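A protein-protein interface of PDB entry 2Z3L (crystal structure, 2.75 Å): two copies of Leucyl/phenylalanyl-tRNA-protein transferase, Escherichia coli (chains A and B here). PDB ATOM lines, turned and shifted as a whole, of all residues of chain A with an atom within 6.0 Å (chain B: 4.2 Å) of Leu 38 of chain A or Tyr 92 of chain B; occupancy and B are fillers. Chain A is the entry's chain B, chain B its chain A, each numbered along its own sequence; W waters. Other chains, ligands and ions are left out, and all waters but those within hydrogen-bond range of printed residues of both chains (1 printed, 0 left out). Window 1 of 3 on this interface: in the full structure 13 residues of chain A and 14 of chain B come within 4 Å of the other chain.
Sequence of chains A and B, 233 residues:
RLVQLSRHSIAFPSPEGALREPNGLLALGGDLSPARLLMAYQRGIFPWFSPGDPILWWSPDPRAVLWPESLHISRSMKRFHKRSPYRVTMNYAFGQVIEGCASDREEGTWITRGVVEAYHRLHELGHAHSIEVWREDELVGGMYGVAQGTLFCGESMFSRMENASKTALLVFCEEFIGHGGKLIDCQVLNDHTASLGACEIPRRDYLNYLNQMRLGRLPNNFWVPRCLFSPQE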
ATOM      1  N   SER A  33      -5.412 -16.825   5.218  1.00  0.00           N
ATOM      2  CA  SER A  33      -6.711 -17.106   5.814  1.00  0.00           C
ATOM      3  C   SER A  33      -7.193 -18.465   5.313  1.00  0.00           C
ATOM      4  O   SER A  33      -6.823 -18.909   4.226  1.00  0.00           O
ATOM      5  CB  SER A  33      -7.737 -16.029   5.430  1.00  0.00           C
ATOM      6  OG  SER A  33      -8.190 -16.177   4.090  1.00  0.00           O
ATOM      7  N   PRO A  34      -8.029 -19.142   6.107  1.00  0.00           N
ATOM      8  CA  PRO A  34      -8.588 -20.455   5.785  1.00  0.00           C
ATOM      9  C   PRO A  34      -9.214 -20.520   4.392  1.00  0.00           C
ATOM     10  O   PRO A  34      -8.933 -21.433   3.604  1.00  0.00           O
ATOM     11  CB  PRO A  34      -9.626 -20.649   6.880  1.00  0.00           C
ATOM     12  CG  PRO A  34      -9.001 -19.962   8.036  1.00  0.00           C
ATOM     13  CD  PRO A  34      -8.498 -18.690   7.428  1.00  0.00           C
ATOM     14  N   ALA A  35     -10.064 -19.542   4.100  1.00  0.00           N
ATOM     15  CA  ALA A  35     -10.760 -19.471   2.823  1.00  0.00           C
ATOM     16  C   ALA A  35      -9.806 -19.409   1.643  1.00  0.00           C
ATOM     17  O   ALA A  35      -9.973 -20.127   0.655  1.00  0.00           O
ATOM     18  CB  ALA A  35     -11.685 -18.256   2.806  1.00  0.00           C
ATOM     19  N   ARG A  36      -8.812 -18.539   1.745  1.00  0.00           N
ATOM     20  CA  ARG A  36      -7.853 -18.386   0.668  1.00  0.00           C
ATOM     21  C   ARG A  36      -7.002 -19.646   0.495  1.00  0.00           C
ATOM     22  O   ARG A  36      -6.710 -20.056  -0.634  1.00  0.00           O
ATOM     23  CB  ARG A  36      -6.979 -17.164   0.929  1.00  0.00           C
ATOM     24  CG  ARG A  36      -5.862 -16.984  -0.060  1.00  0.00           C
ATOM     25  CD  ARG A  36      -5.318 -15.593   0.058  1.00  0.00           C
ATOM     26  NE  ARG A  36      -6.205 -14.646  -0.601  1.00  0.00           N
ATOM     27  CZ  ARG A  36      -6.394 -13.397  -0.196  1.00  0.00           C
ATOM     28  NH1 ARG A  36      -5.763 -12.944   0.876  1.00  0.00           N
ATOM     29  NH2 ARG A  36      -7.204 -12.595  -0.869  1.00  0.00           N
ATOM     30  N   LEU A  37      -6.619 -20.271   1.605  1.00  0.00           N
ATOM     31  CA  LEU A  37      -5.823 -21.477   1.519  1.00  0.00           C
ATOM     32  C   LEU A  37      -6.599 -22.633   0.903  1.00  0.00           C
ATOM     33  O   LEU A  37      -6.077 -23.341   0.035  1.00  0.00           O
ATOM     34  CB  LEU A  37      -5.304 -21.876   2.895  1.00  0.00           C
ATOM     35  CG  LEU A  37      -4.081 -21.098   3.388  1.00  0.00           C
ATOM     36  CD1 LEU A  37      -3.655 -21.691   4.717  1.00  0.00           C
ATOM     37  CD2 LEU A  37      -2.933 -21.163   2.358  1.00  0.00           C
ATOM     38  N   LEU A  38      -7.838 -22.838   1.340  1.00  0.00           N
ATOM     39  CA  LEU A  38      -8.622 -23.936   0.782  1.00  0.00           C
ATOM     40  C   LEU A  38      -8.934 -23.682  -0.673  1.00  0.00           C
ATOM     41  O   LEU A  38      -9.121 -24.614  -1.455  1.00  0.00           O
ATOM     42  CB  LEU A  38      -9.924 -24.138   1.545  1.00  0.00           C
ATOM     43  CG  LEU A  38      -9.775 -25.030   2.768  1.00  0.00           C
ATOM     44  CD1 LEU A  38      -8.829 -24.373   3.740  1.00  0.00           C
ATOM     45  CD2 LEU A  38     -11.125 -25.254   3.411  1.00  0.00           C
ATOM     46  N   MET A  39      -9.000 -22.407  -1.031  1.00  0.00           N
ATOM     47  CA  MET A  39      -9.271 -22.030  -2.398  1.00  0.00           C
ATOM     48  C   MET A  39      -8.063 -22.391  -3.263  1.00  0.00           C
ATOM     49  O   MET A  39      -8.202 -22.972  -4.329  1.00  0.00           O
ATOM     50  CB  MET A  39      -9.574 -20.536  -2.455  1.00  0.00           C
ATOM     51  CG  MET A  39     -11.060 -20.225  -2.363  1.00  0.00           C
ATOM     52  SD  MET A  39     -11.936 -20.687  -3.894  1.00  0.00           S
ATOM     53  CE  MET A  39     -10.900 -19.827  -5.163  1.00  0.00           C
ATOM     54  N   ALA A  40      -6.874 -22.067  -2.777  1.00  0.00           N
ATOM     55  CA  ALA A  40      -5.638 -22.367  -3.488  1.00  0.00           C
ATOM     56  C   ALA A  40      -5.392 -23.873  -3.628  1.00  0.00           C
ATOM     57  O   ALA A  40      -4.999 -24.340  -4.697  1.00  0.00           O
ATOM     58  CB  ALA A  40      -4.453 -21.708  -2.771  1.00  0.00           C
ATOM     59  N   TYR A  41      -5.620 -24.631  -2.558  1.00  0.00           N
ATOM     60  CA  TYR A  41      -5.393 -26.078  -2.598  1.00  0.00           C
ATOM     61  C   TYR A  41      -6.345 -26.862  -3.488  1.00  0.00           C
ATOM     62  O   TYR A  41      -6.008 -27.959  -3.935  1.00  0.00           O
ATOM     63  CB  TYR A  41      -5.416 -26.664  -1.186  1.00  0.00           C
ATOM     64  CG  TYR A  41      -4.090 -26.536  -0.474  1.00  0.00           C
ATOM     65  CD1 TYR A  41      -3.103 -27.508  -0.611  1.00  0.00           C
ATOM     66  CD2 TYR A  41      -3.797 -25.408   0.289  1.00  0.00           C
ATOM     67  CE1 TYR A  41      -1.856 -27.359  -0.008  1.00  0.00           C
ATOM     68  CE2 TYR A  41      -2.556 -25.248   0.894  1.00  0.00           C
ATOM     69  CZ  TYR A  41      -1.589 -26.222   0.742  1.00  0.00           C
ATOM     70  OH  TYR A  41      -0.360 -26.046   1.338  1.00  0.00           O
ATOM     71  N   GLN A  42      -7.528 -26.311  -3.752  1.00  0.00           N
ATOM     72  CA  GLN A  42      -8.479 -27.003  -4.605  1.00  0.00           C
ATOM     73  C   GLN A  42      -8.240 -26.610  -6.057  1.00  0.00           C
ATOM     74  O   GLN A  42      -8.878 -27.141  -6.968  1.00  0.00           O
ATOM     75  CB  GLN A  42      -9.916 -26.689  -4.193  1.00  0.00           C
ATOM     76  CG  GLN A  42     -10.404 -25.309  -4.555  1.00  0.00           C
ATOM     77  CD  GLN A  42     -11.884 -25.128  -4.246  1.00  0.00           C
ATOM     78  OE1 GLN A  42     -12.743 -25.821  -4.804  1.00  0.00           O
ATOM     79  NE2 GLN A  42     -12.189 -24.198  -3.346  1.00  0.00           N
ATOM     80  N   ARG A  43      -7.298 -25.689  -6.261  1.00  0.00           N
ATOM     81  CA  ARG A  43      -6.940 -25.215  -7.601  1.00  0.00           C
ATOM     82  C   ARG A  43      -5.508 -25.640  -7.945  1.00  0.00           C
ATOM     83  O   ARG A  43      -4.982 -25.272  -8.997  1.00  0.00           O
ATOM     84  CB  ARG A  43      -7.039 -23.685  -7.679  1.00  0.00           C
ATOM     85  CG  ARG A  43      -8.350 -23.116  -7.161  1.00  0.00           C
ATOM     86  CD  ARG A  43      -9.394 -22.919  -8.239  1.00  0.00           C
ATOM     87  NE  ARG A  43      -9.181 -21.670  -8.968  1.00  0.00           N
ATOM     88  CZ  ARG A  43      -8.294 -21.507  -9.948  1.00  0.00           C
ATOM     89  NH1 ARG A  43      -7.527 -22.520 -10.336  1.00  0.00           N
ATOM     90  NH2 ARG A  43      -8.174 -20.328 -10.544  1.00  0.00           N
ATOM     91  N   LEU A 122      -6.152 -24.641   9.960  1.00  0.00           N
ATOM     92  CA  LEU A 122      -6.743 -25.588   9.023  1.00  0.00           C
ATOM     93  C   LEU A 122      -6.922 -26.892   9.776  1.00  0.00           C
ATOM     94  O   LEU A 122      -7.907 -27.601   9.593  1.00  0.00           O
ATOM     95  CB  LEU A 122      -5.835 -25.838   7.814  1.00  0.00           C
ATOM     96  CG  LEU A 122      -5.781 -24.776   6.722  1.00  0.00           C
ATOM     97  CD1 LEU A 122      -5.004 -25.317   5.554  1.00  0.00           C
ATOM     98  CD2 LEU A 122      -7.189 -24.405   6.279  1.00  0.00           C
ATOM     99  N   LEU A 125     -10.012 -26.794  11.582  1.00  0.00           N
ATOM    100  CA  LEU A 125     -11.208 -26.816  10.759  1.00  0.00           C
ATOM    101  C   LEU A 125     -11.405 -28.152  10.015  1.00  0.00           C
ATOM    102  O   LEU A 125     -12.327 -28.296   9.201  1.00  0.00           O
ATOM    103  CB  LEU A 125     -11.184 -25.631   9.791  1.00  0.00           C
ATOM    104  CG  LEU A 125     -11.282 -24.263  10.499  1.00  0.00           C
ATOM    105  CD1 LEU A 125     -11.170 -23.129   9.483  1.00  0.00           C
ATOM    106  CD2 LEU A 125     -12.606 -24.162  11.256  1.00  0.00           C
ATOM    107  N   GLY A 126     -10.536 -29.123  10.303  1.00  0.00           N
ATOM    108  CA  GLY A 126     -10.636 -30.442   9.694  1.00  0.00           C
ATOM    109  C   GLY A 126      -9.935 -30.728   8.378  1.00  0.00           C
ATOM    110  O   GLY A 126     -10.231 -31.738   7.738  1.00  0.00           O
ATOM    111  N   HIS A 127      -8.993 -29.886   7.966  1.00  0.00           N
ATOM    112  CA  HIS A 127      -8.311 -30.124   6.695  1.00  0.00           C
ATOM    113  C   HIS A 127      -6.824 -30.407   6.770  1.00  0.00           C
ATOM    114  O   HIS A 127      -6.260 -31.005   5.858  1.00  0.00           O
ATOM    115  CB  HIS A 127      -8.532 -28.952   5.741  1.00  0.00           C
ATOM    116  CG  HIS A 127      -9.970 -28.600   5.557  1.00  0.00           C
ATOM    117  ND1 HIS A 127     -10.635 -27.735   6.399  1.00  0.00           N
ATOM    118  CD2 HIS A 127     -10.879 -29.019   4.648  1.00  0.00           C
ATOM    119  CE1 HIS A 127     -11.893 -27.635   6.015  1.00  0.00           C
ATOM    120  NE2 HIS A 127     -12.067 -28.405   4.955  1.00  0.00           N
ATOM    121  N   GLN A 148      -7.293 -33.544   0.590  1.00  0.00           N
ATOM    122  CA  GLN A 148      -8.068 -33.036  -0.523  1.00  0.00           C
ATOM    123  C   GLN A 148      -8.878 -34.223  -1.049  1.00  0.00           C
ATOM    124  O   GLN A 148      -8.771 -34.598  -2.217  1.00  0.00           O
ATOM    125  CB  GLN A 148      -7.094 -32.554  -1.598  1.00  0.00           C
ATOM    126  CG  GLN A 148      -7.572 -31.422  -2.483  1.00  0.00           C
ATOM    127  CD  GLN A 148      -7.820 -30.152  -1.707  1.00  0.00           C
ATOM    128  OE1 GLN A 148      -7.178 -29.912  -0.696  1.00  0.00           O
ATOM    129  NE2 GLN A 148      -8.749 -29.326  -2.182  1.00  0.00           N
ATOM    130  N   ARG A 214     -10.547 -34.709  -5.192  1.00  0.00           N
ATOM    131  CA  ARG A 214     -11.065 -33.805  -4.165  1.00  0.00           C
ATOM    132  C   ARG A 214     -12.524 -34.042  -3.814  1.00  0.00           C
ATOM    133  O   ARG A 214     -12.971 -33.652  -2.736  1.00  0.00           O
ATOM    134  CB  ARG A 214     -10.855 -32.336  -4.542  1.00  0.00           C
ATOM    135  CG  ARG A 214     -11.345 -31.924  -5.904  1.00  0.00           C
ATOM    136  CD  ARG A 214     -11.039 -30.446  -6.137  1.00  0.00           C
ATOM    137  NE  ARG A 214     -12.064 -29.578  -5.566  1.00  0.00           N
ATOM    138  CZ  ARG A 214     -13.194 -29.264  -6.190  1.00  0.00           C
ATOM    139  NH1 ARG A 214     -13.438 -29.742  -7.405  1.00  0.00           N
ATOM    140  NH2 ARG A 214     -14.084 -28.479  -5.597  1.00  0.00           N
ATOM    141  N   THR B  89     -19.700 -22.266   0.455  1.00  0.00           N
ATOM    142  CA  THR B  89     -18.971 -23.522   0.540  1.00  0.00           C
ATOM    143  C   THR B  89     -19.631 -24.469   1.523  1.00  0.00           C
ATOM    144  O   THR B  89     -20.430 -24.059   2.364  1.00  0.00           O
ATOM    145  CB  THR B  89     -17.514 -23.308   1.006  1.00  0.00           C
ATOM    146  OG1 THR B  89     -17.509 -22.823   2.352  1.00  0.00           O
ATOM    147  CG2 THR B  89     -16.807 -22.298   0.121  1.00  0.00           C
ATOM    148  N   MET B  90     -19.288 -25.745   1.408  1.00  0.00           N
ATOM    149  CA  MET B  90     -19.826 -26.752   2.304  1.00  0.00           C
ATOM    150  C   MET B  90     -18.694 -27.324   3.120  1.00  0.00           C
ATOM    151  O   MET B  90     -17.638 -27.622   2.592  1.00  0.00           O
ATOM    152  CB  MET B  90     -20.490 -27.871   1.521  1.00  0.00           C
ATOM    153  CG  MET B  90     -21.182 -28.888   2.400  1.00  0.00           C
ATOM    154  SD  MET B  90     -21.707 -30.300   1.424  1.00  0.00           S
ATOM    155  CE  MET B  90     -23.372 -29.796   0.923  1.00  0.00           C
ATOM    156  N   ASN B  91     -18.932 -27.461   4.415  1.00  0.00           N
ATOM    157  CA  ASN B  91     -17.963 -28.007   5.356  1.00  0.00           C
ATOM    158  C   ASN B  91     -16.544 -27.469   5.293  1.00  0.00           C
ATOM    159  O   ASN B  91     -15.600 -28.216   5.523  1.00  0.00           O
ATOM    160  CB  ASN B  91     -17.920 -29.528   5.251  1.00  0.00           C
ATOM    161  CG  ASN B  91     -19.206 -30.170   5.719  1.00  0.00           C
ATOM    162  OD1 ASN B  91     -19.704 -29.871   6.807  1.00  0.00           O
ATOM    163  ND2 ASN B  91     -19.758 -31.062   4.898  1.00  0.00           N
ATOM    164  N   TYR B  92     -16.395 -26.180   4.989  1.00  0.00           N
ATOM    165  CA  TYR B  92     -15.077 -25.552   4.939  1.00  0.00           C
ATOM    166  C   TYR B  92     -14.664 -25.194   6.352  1.00  0.00           C
ATOM    167  O   TYR B  92     -13.544 -25.470   6.764  1.00  0.00           O
ATOM    168  CB  TYR B  92     -15.106 -24.269   4.104  1.00  0.00           C
ATOM    169  CG  TYR B  92     -14.552 -24.415   2.708  1.00  0.00           C
ATOM    170  CD1 TYR B  92     -14.602 -25.638   2.042  1.00  0.00           C
ATOM    171  CD2 TYR B  92     -14.035 -23.317   2.020  1.00  0.00           C
ATOM    172  CE1 TYR B  92     -14.158 -25.765   0.725  1.00  0.00           C
ATOM    173  CE2 TYR B  92     -13.586 -23.434   0.694  1.00  0.00           C
ATOM    174  CZ  TYR B  92     -13.655 -24.665   0.056  1.00  0.00           C
ATOM    175  OH  TYR B  92     -13.238 -24.806  -1.248  1.00  0.00           O
ATOM    176  N   ALA B  93     -15.584 -24.583   7.094  1.00  0.00           N
ATOM    177  CA  ALA B  93     -15.301 -24.162   8.456  1.00  0.00           C
ATOM    178  C   ALA B  93     -16.468 -24.367   9.415  1.00  0.00           C
ATOM    179  O   ALA B  93     -17.076 -23.396   9.870  1.00  0.00           O
ATOM    180  CB  ALA B  93     -14.875 -22.683   8.459  1.00  0.00           C
ATOM    181  N   PHE B  94     -16.764 -25.622   9.739  1.00  0.00           N
ATOM    182  CA  PHE B  94     -17.863 -25.935  10.655  1.00  0.00           C
ATOM    183  C   PHE B  94     -17.687 -25.158  11.958  1.00  0.00           C
ATOM    184  O   PHE B  94     -18.614 -24.501  12.443  1.00  0.00           O
ATOM    185  CB  PHE B  94     -17.889 -27.433  10.966  1.00  0.00           C
ATOM    186  CG  PHE B  94     -19.078 -27.870  11.784  1.00  0.00           C
ATOM    187  CD1 PHE B  94     -20.284 -28.196  11.169  1.00  0.00           C
ATOM    188  CD2 PHE B  94     -18.992 -27.961  13.176  1.00  0.00           C
ATOM    189  CE1 PHE B  94     -21.390 -28.607  11.930  1.00  0.00           C
ATOM    190  CE2 PHE B  94     -20.095 -28.369  13.943  1.00  0.00           C
ATOM    191  CZ  PHE B  94     -21.295 -28.694  13.319  1.00  0.00           C
ATOM    192  N   GLU B 132     -21.082 -22.520   4.498  1.00  0.00           N
ATOM    193  CA  GLU B 132     -20.474 -21.226   4.800  1.00  0.00           C
ATOM    194  C   GLU B 132     -20.771 -20.202   3.723  1.00  0.00           C
ATOM    195  O   GLU B 132     -20.822 -20.545   2.543  1.00  0.00           O
ATOM    196  CB  GLU B 132     -18.950 -21.346   4.920  1.00  0.00           C
ATOM    197  CG  GLU B 132     -18.456 -22.286   6.011  1.00  0.00           C
ATOM    198  CD  GLU B 132     -18.462 -23.748   5.593  1.00  0.00           C
ATOM    199  OE1 GLU B 132     -18.631 -24.606   6.478  1.00  0.00           O
ATOM    200  OE2 GLU B 132     -18.286 -24.047   4.392  1.00  0.00           O
ATOM    201  N   ARG B 226     -16.543 -28.659  -0.274  1.00  0.00           N
ATOM    202  CA  ARG B 226     -16.372 -28.062  -1.598  1.00  0.00           C
ATOM    203  C   ARG B 226     -17.038 -26.699  -1.691  1.00  0.00           C
ATOM    204  O   ARG B 226     -17.619 -26.195  -0.729  1.00  0.00           O
ATOM    205  CB  ARG B 226     -16.989 -28.955  -2.663  1.00  0.00           C
ATOM    206  CG  ARG B 226     -18.472 -29.216  -2.457  1.00  0.00           C
ATOM    207  CD  ARG B 226     -18.726 -30.698  -2.539  1.00  0.00           C
ATOM    208  NE  ARG B 226     -20.088 -31.098  -2.207  1.00  0.00           N
ATOM    209  CZ  ARG B 226     -21.124 -30.927  -3.012  1.00  0.00           C
ATOM    210  NH1 ARG B 226     -20.942 -30.349  -4.197  1.00  0.00           N
ATOM    211  NH2 ARG B 226     -22.327 -31.365  -2.647  1.00  0.00           N
HETATM  212  O   HOH W   1     -14.767 -27.501   9.270  1.00  0.00           O
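The side-chain hydroxyl (OH) of Tyr 92 of chain B lies within hydrogen-bond range of the side-chain amide nitrogen (NE2) of Gln 42 of chain A, 2.4 Å away.
The backbone NH of Asn 91 of chain B lies within hydrogen-bond range of the side-chain carboxylate of Glu 132 of chain B (3.5 Å).
The backbone NH of Tyr 92 of chain B lies within hydrogen-bond range of the side-chain carboxylate of Glu 132 of chain B (2.9 Å).
The backbone NH (N) of Ala 93 of chain B sits at hydrogen-bond distance from the side-chain carboxylate (OE1) of Glu 132 of chain B (3.1 Å).
OE1 of Gln 42 of chain A is in hydrogen-bond range of NH2 of Arg 214 of chain A, at 3.1 Å.
The backbone carbonyl oxygen (O) of Leu 122 of chain A lies within hydrogen-bond range of the backbone NH (N) of His 127 of chain A, at 3.0 Å.
O of Leu 125 of chain A lies close to ND1 of His 127 of chain A (3.3 Å).
Among the printed residues, pairs that only touch across the chains: His 127 of chain A with Tyr 92 of chain B, His 127 of chain A with Asn 91 of chain B, Leu 38 of chain A with Tyr 92 of chain B, Leu 125 of chain A with Tyr 92 of chain B and Leu 125 of chain A with Ala 93 of chain B.
Of chain A, only Leu 38, Gln 42, Leu 125 and His 127 come within 4 Å of Tyr 92 of chain B.
Printed residues of chain B within 4 Å of Leu 125 of chain A: Tyr 92 (3.8 Å) and Ala 93 (3.9 Å).
Printed residues of chain B within 4 Å of Gln 42 of chain A: Tyr 92.
Printed residues of chain A within 4 Å of Asn 91 of chain B: His 127 (3.6 Å).
Of the printed residues of chain A, Ala 93 of chain B touches Leu 125 (3.9 Å).
The nearest printed residue of chain A that does not touch Tyr 92 of chain B is Met 39 of chain A (4.9 Å).
Of the 8 printed residues of chain B, 3 touch a printed residue of chain A.
Hydrophobic or aromatic side chains of chain B that line the printed part of chain A: Tyr 92 and Ala 93.
Of the 17 printed residues of chain A, 4 touch a printed residue of chain B.
Printed residues of chain A that touch a printed residue of chain B: Leu 38, Gln 42, Leu 125 and His 127.
No position is printed for both chains.
Of the 6 pairs that touch across the chains among the printed residues, none has its exchanged pair printed and touching as well.
Water W1 lies within hydrogen-bond range of O of Leu 125 of chain A, N of Phe 94 of chain B and O of Tyr 92 of chain B.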
